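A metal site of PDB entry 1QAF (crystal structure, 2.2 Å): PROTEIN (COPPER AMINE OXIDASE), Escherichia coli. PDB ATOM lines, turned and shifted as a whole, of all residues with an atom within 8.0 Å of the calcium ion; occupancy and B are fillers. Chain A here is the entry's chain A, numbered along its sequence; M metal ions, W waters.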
ATOM      1  N   GLU A 568     -15.628   0.723  10.185  1.00  0.00           N
ATOM      2  CA  GLU A 568     -16.085   1.889   9.447  1.00  0.00           C
ATOM      3  C   GLU A 568     -17.397   2.487   9.922  1.00  0.00           C
ATOM      4  O   GLU A 568     -17.508   3.712   9.891  1.00  0.00           O
ATOM      5  CB  GLU A 568     -16.143   1.705   7.919  1.00  0.00           C
ATOM      6  CG  GLU A 568     -14.877   1.090   7.365  1.00  0.00           C
ATOM      7  CD  GLU A 568     -15.003   0.481   5.973  1.00  0.00           C
ATOM      8  OE1 GLU A 568     -15.890  -0.338   5.644  1.00  0.00           O
ATOM      9  OE2 GLU A 568     -14.119   0.871   5.183  1.00  0.00           O
ATOM     10  N   VAL A 635     -13.996   7.387   8.354  1.00  0.00           N
ATOM     11  CA  VAL A 635     -12.713   6.699   8.197  1.00  0.00           C
ATOM     12  C   VAL A 635     -13.041   5.399   7.426  1.00  0.00           C
ATOM     13  O   VAL A 635     -13.888   4.616   7.889  1.00  0.00           O
ATOM     14  CB  VAL A 635     -11.888   6.412   9.459  1.00  0.00           C
ATOM     15  CG1 VAL A 635     -10.500   5.862   9.172  1.00  0.00           C
ATOM     16  CG2 VAL A 635     -11.940   7.696  10.287  1.00  0.00           C
ATOM     17  N   THR A 636     -12.422   5.208   6.239  1.00  0.00           N
ATOM     18  CA  THR A 636     -12.741   3.977   5.478  1.00  0.00           C
ATOM     19  C   THR A 636     -11.433   3.293   5.142  1.00  0.00           C
ATOM     20  O   THR A 636     -10.422   4.004   5.276  1.00  0.00           O
ATOM     21  CB  THR A 636     -13.438   4.304   4.134  1.00  0.00           C
ATOM     22  OG1 THR A 636     -12.646   5.251   3.363  1.00  0.00           O
ATOM     23  CG2 THR A 636     -14.813   4.885   4.489  1.00  0.00           C
ATOM     24  N   ARG A 637     -11.488   2.030   4.732  1.00  0.00           N
ATOM     25  CA  ARG A 637     -10.238   1.355   4.340  1.00  0.00           C
ATOM     26  C   ARG A 637      -9.820   1.927   2.974  1.00  0.00           C
ATOM     27  O   ARG A 637     -10.656   2.246   2.112  1.00  0.00           O
ATOM     28  CB  ARG A 637     -10.380  -0.151   4.169  1.00  0.00           C
ATOM     29  CG  ARG A 637     -11.017  -0.866   5.347  1.00  0.00           C
ATOM     30  CD  ARG A 637     -10.962  -2.353   5.019  1.00  0.00           C
ATOM     31  NE  ARG A 637     -10.286  -3.031   6.097  1.00  0.00           N
ATOM     32  CZ  ARG A 637      -9.220  -3.803   6.066  1.00  0.00           C
ATOM     33  NH1 ARG A 637      -8.561  -4.185   4.999  1.00  0.00           N
ATOM     34  NH2 ARG A 637      -8.862  -4.217   7.288  1.00  0.00           N
ATOM     35  N   TYR A 638      -8.524   2.146   2.736  1.00  0.00           N
ATOM     36  CA  TYR A 638      -8.000   2.690   1.500  1.00  0.00           C
ATOM     37  C   TYR A 638      -8.365   1.775   0.332  1.00  0.00           C
ATOM     38  O   TYR A 638      -8.180   0.582   0.549  1.00  0.00           O
ATOM     39  CB  TYR A 638      -6.450   2.722   1.548  1.00  0.00           C
ATOM     40  CG  TYR A 638      -5.894   3.109   0.182  1.00  0.00           C
ATOM     41  CD1 TYR A 638      -5.962   4.384  -0.385  1.00  0.00           C
ATOM     42  CD2 TYR A 638      -5.272   2.128  -0.579  1.00  0.00           C
ATOM     43  CE1 TYR A 638      -5.473   4.676  -1.640  1.00  0.00           C
ATOM     44  CE2 TYR A 638      -4.747   2.373  -1.836  1.00  0.00           C
ATOM     45  CZ  TYR A 638      -4.870   3.654  -2.348  1.00  0.00           C
ATOM     46  OH  TYR A 638      -4.363   3.933  -3.583  1.00  0.00           O
ATOM     47  N   HIS A 639      -8.811   2.364  -0.742  1.00  0.00           N
ATOM     48  CA  HIS A 639      -9.214   1.714  -1.999  1.00  0.00           C
ATOM     49  C   HIS A 639      -9.006   2.812  -3.048  1.00  0.00           C
ATOM     50  O   HIS A 639      -9.448   3.959  -3.036  1.00  0.00           O
ATOM     51  CB  HIS A 639     -10.592   1.043  -1.986  1.00  0.00           C
ATOM     52  CG  HIS A 639     -10.800  -0.124  -1.048  1.00  0.00           C
ATOM     53  ND1 HIS A 639     -11.922  -0.307  -0.225  1.00  0.00           N
ATOM     54  CD2 HIS A 639     -10.024  -1.210  -0.770  1.00  0.00           C
ATOM     55  CE1 HIS A 639     -11.823  -1.430   0.490  1.00  0.00           C
ATOM     56  NE2 HIS A 639     -10.656  -1.983   0.177  1.00  0.00           N
ATOM     57  N   GLU A 642     -12.203   4.884  -4.608  1.00  0.00           N
ATOM     58  CA  GLU A 642     -13.196   5.446  -3.675  1.00  0.00           C
ATOM     59  C   GLU A 642     -12.594   6.835  -3.469  1.00  0.00           C
ATOM     60  O   GLU A 642     -11.682   6.916  -2.643  1.00  0.00           O
ATOM     61  CB  GLU A 642     -13.212   4.655  -2.356  1.00  0.00           C
ATOM     62  CG  GLU A 642     -13.564   3.197  -2.655  1.00  0.00           C
ATOM     63  CD  GLU A 642     -14.030   2.470  -1.409  1.00  0.00           C
ATOM     64  OE1 GLU A 642     -13.555   2.704  -0.275  1.00  0.00           O
ATOM     65  OE2 GLU A 642     -14.952   1.650  -1.519  1.00  0.00           O
ATOM     66  N   LEU A 659     -19.602   7.861   0.235  1.00  0.00           N
ATOM     67  CA  LEU A 659     -19.182   7.401   1.558  1.00  0.00           C
ATOM     68  C   LEU A 659     -20.160   6.386   2.136  1.00  0.00           C
ATOM     69  O   LEU A 659     -19.662   5.529   2.843  1.00  0.00           O
ATOM     70  CB  LEU A 659     -18.982   8.607   2.485  1.00  0.00           C
ATOM     71  CG  LEU A 659     -17.623   9.332   2.376  1.00  0.00           C
ATOM     72  CD1 LEU A 659     -17.592  10.642   3.197  1.00  0.00           C
ATOM     73  CD2 LEU A 659     -16.531   8.421   2.929  1.00  0.00           C
ATOM     74  N   GLN A 661     -21.801   4.115   0.427  1.00  0.00           N
ATOM     75  CA  GLN A 661     -21.426   2.837  -0.160  1.00  0.00           C
ATOM     76  C   GLN A 661     -20.047   2.424   0.333  1.00  0.00           C
ATOM     77  O   GLN A 661     -19.952   1.225   0.579  1.00  0.00           O
ATOM     78  CB  GLN A 661     -21.241   3.039  -1.686  1.00  0.00           C
ATOM     79  CG  GLN A 661     -20.778   1.910  -2.608  1.00  0.00           C
ATOM     80  CD  GLN A 661     -20.630   2.220  -4.102  1.00  0.00           C
ATOM     81  OE1 GLN A 661     -21.485   2.584  -4.910  1.00  0.00           O
ATOM     82  NE2 GLN A 661     -19.403   2.112  -4.589  1.00  0.00           N
ATOM     83  N   TYR A 662     -19.093   3.369   0.454  1.00  0.00           N
ATOM     84  CA  TYR A 662     -17.758   2.963   0.893  1.00  0.00           C
ATOM     85  C   TYR A 662     -17.635   2.375   2.276  1.00  0.00           C
ATOM     86  O   TYR A 662     -16.741   1.593   2.540  1.00  0.00           O
ATOM     87  CB  TYR A 662     -16.788   4.157   0.837  1.00  0.00           C
ATOM     88  CG  TYR A 662     -16.734   4.925  -0.460  1.00  0.00           C
ATOM     89  CD1 TYR A 662     -16.885   4.290  -1.706  1.00  0.00           C
ATOM     90  CD2 TYR A 662     -16.469   6.296  -0.447  1.00  0.00           C
ATOM     91  CE1 TYR A 662     -16.836   4.999  -2.900  1.00  0.00           C
ATOM     92  CE2 TYR A 662     -16.417   7.031  -1.627  1.00  0.00           C
ATOM     93  CZ  TYR A 662     -16.610   6.375  -2.841  1.00  0.00           C
ATOM     94  OH  TYR A 662     -16.535   7.077  -4.013  1.00  0.00           O
ATOM     95  N   SER A 663     -18.536   2.759   3.164  1.00  0.00           N
ATOM     96  CA  SER A 663     -18.554   2.277   4.537  1.00  0.00           C
ATOM     97  C   SER A 663     -19.576   1.173   4.751  1.00  0.00           C
ATOM     98  O   SER A 663     -19.491   0.489   5.771  1.00  0.00           O
ATOM     99  CB  SER A 663     -18.821   3.479   5.471  1.00  0.00           C
ATOM    100  OG  SER A 663     -20.074   4.068   5.129  1.00  0.00           O
ATOM    101  N   LYS A 664     -20.490   1.048   3.797  1.00  0.00           N
ATOM    102  CA  LYS A 664     -21.573   0.074   3.789  1.00  0.00           C
ATOM    103  C   LYS A 664     -21.221  -1.279   4.428  1.00  0.00           C
ATOM    104  O   LYS A 664     -21.879  -1.767   5.331  1.00  0.00           O
ATOM    105  CB  LYS A 664     -22.004  -0.247   2.343  1.00  0.00           C
ATOM    106  CG  LYS A 664     -23.251  -1.057   2.126  1.00  0.00           C
ATOM    107  CD  LYS A 664     -24.502  -0.381   1.593  1.00  0.00           C
ATOM    108  CE  LYS A 664     -25.501  -1.303   0.912  1.00  0.00           C
ATOM    109  NZ  LYS A 664     -25.430  -2.709   1.390  1.00  0.00           N
ATOM    110  N   ASP A 665     -20.158  -1.876   3.935  1.00  0.00           N
ATOM    111  CA  ASP A 665     -19.680  -3.161   4.395  1.00  0.00           C
ATOM    112  C   ASP A 665     -19.124  -3.133   5.814  1.00  0.00           C
ATOM    113  O   ASP A 665     -18.786  -4.236   6.294  1.00  0.00           O
ATOM    114  CB  ASP A 665     -18.667  -3.758   3.438  1.00  0.00           C
ATOM    115  CG  ASP A 665     -19.264  -4.200   2.119  1.00  0.00           C
ATOM    116  OD1 ASP A 665     -20.480  -4.524   2.179  1.00  0.00           O
ATOM    117  OD2 ASP A 665     -18.608  -4.256   1.057  1.00  0.00           O
ATOM    118  N   ASN A 666     -19.007  -1.947   6.434  1.00  0.00           N
ATOM    119  CA  ASN A 666     -18.473  -1.897   7.812  1.00  0.00           C
ATOM    120  C   ASN A 666     -17.206  -2.730   7.999  1.00  0.00           C
ATOM    121  O   ASN A 666     -17.188  -3.678   8.781  1.00  0.00           O
ATOM    122  CB  ASN A 666     -19.454  -2.523   8.811  1.00  0.00           C
ATOM    123  CG  ASN A 666     -19.319  -2.074  10.243  1.00  0.00           C
ATOM    124  OD1 ASN A 666     -19.894  -2.592  11.222  1.00  0.00           O
ATOM    125  ND2 ASN A 666     -18.564  -0.997  10.472  1.00  0.00           N
ATOM    126  N   GLU A 667     -16.128  -2.434   7.279  1.00  0.00           N
ATOM    127  CA  GLU A 667     -14.943  -3.254   7.449  1.00  0.00           C
ATOM    128  C   GLU A 667     -14.126  -2.763   8.638  1.00  0.00           C
ATOM    129  O   GLU A 667     -14.359  -1.663   9.185  1.00  0.00           O
ATOM    130  CB  GLU A 667     -14.113  -3.253   6.150  1.00  0.00           C
ATOM    131  CG  GLU A 667     -14.750  -3.675   4.829  1.00  0.00           C
ATOM    132  CD  GLU A 667     -13.854  -3.528   3.599  1.00  0.00           C
ATOM    133  OE1 GLU A 667     -13.908  -2.439   2.966  1.00  0.00           O
ATOM    134  OE2 GLU A 667     -13.071  -4.433   3.233  1.00  0.00           O
ATOM    135  N   SER A 668     -13.154  -3.579   9.008  1.00  0.00           N
ATOM    136  CA  SER A 668     -12.268  -3.308  10.112  1.00  0.00           C
ATOM    137  C   SER A 668     -11.224  -2.235   9.845  1.00  0.00           C
ATOM    138  O   SER A 668     -10.581  -2.176   8.798  1.00  0.00           O
ATOM    139  CB  SER A 668     -11.538  -4.609  10.466  1.00  0.00           C
ATOM    140  OG  SER A 668     -10.251  -4.390  11.019  1.00  0.00           O
ATOM    141  N   LEU A 669     -11.036  -1.395  10.860  1.00  0.00           N
ATOM    142  CA  LEU A 669     -10.078  -0.309  10.768  1.00  0.00           C
ATOM    143  C   LEU A 669      -8.946  -0.585  11.751  1.00  0.00           C
ATOM    144  O   LEU A 669      -8.281   0.348  12.183  1.00  0.00           O
ATOM    145  CB  LEU A 669     -10.688   1.058  11.087  1.00  0.00           C
ATOM    146  CG  LEU A 669     -11.657   1.564  10.023  1.00  0.00           C
ATOM    147  CD1 LEU A 669     -12.459   2.804  10.435  1.00  0.00           C
ATOM    148  CD2 LEU A 669     -10.916   1.736   8.719  1.00  0.00           C
HETATM  149 CA    CA M   1     -14.733   0.133   2.874  1.00  0.00          CA
HETATM  150  O   HOH W   1     -17.128  -1.350   3.357  1.00  0.00           O
HETATM  151  O   HOH W   2     -12.933   1.442   1.709  1.00  0.00           O
HETATM  152  O   HOH W   3     -15.240  -0.541   0.210  1.00  0.00           O
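The backbone NH of Arg 637 lies close to the side-chain carboxylate of Glu 568 (2.9 Å). ND2 of Asn 666 sits close to N of Glu 568, at 3.4 Å.
Three residues have an atom within 4 Å of the calcium ion: Glu 568, Tyr 662 and Glu 667. The nearest printed residue that does not touch the calcium ion is His 639 (4.1 Å).
OE2 of Glu 568 binds the calcium ion, 2.5 Å away. O of Tyr 662 binds the calcium ion (2.5 Å). Water W2 is bound to the calcium ion (2.5 Å). The calcium ion is bound by OE1 of Glu 667 (2.7 Å). The calcium ion is bound by water W3, 2.8 Å away. The calcium ion is bound by water W1, 2.9 Å away. Slightly farther from the calcium ion lies OE1 of Glu 568 (3.0 Å).
Water W1 bridges the side-chain carboxylate of Glu 568 (2.8 Å) and the backbone NH of Asp 665 (3.1 Å). Water W2 lies within hydrogen-bond range of the side-chain carboxylate of Glu 642 (2.4 Å), the backbone carbonyl oxygen of Arg 637 (2.4 Å) and a ring nitrogen (ND1) of His 639 (2.8 Å). Water W3 lies within hydrogen-bond range of OE2 of Glu 642 (2.8 Å) and ND1 of His 639 (3.4 Å).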
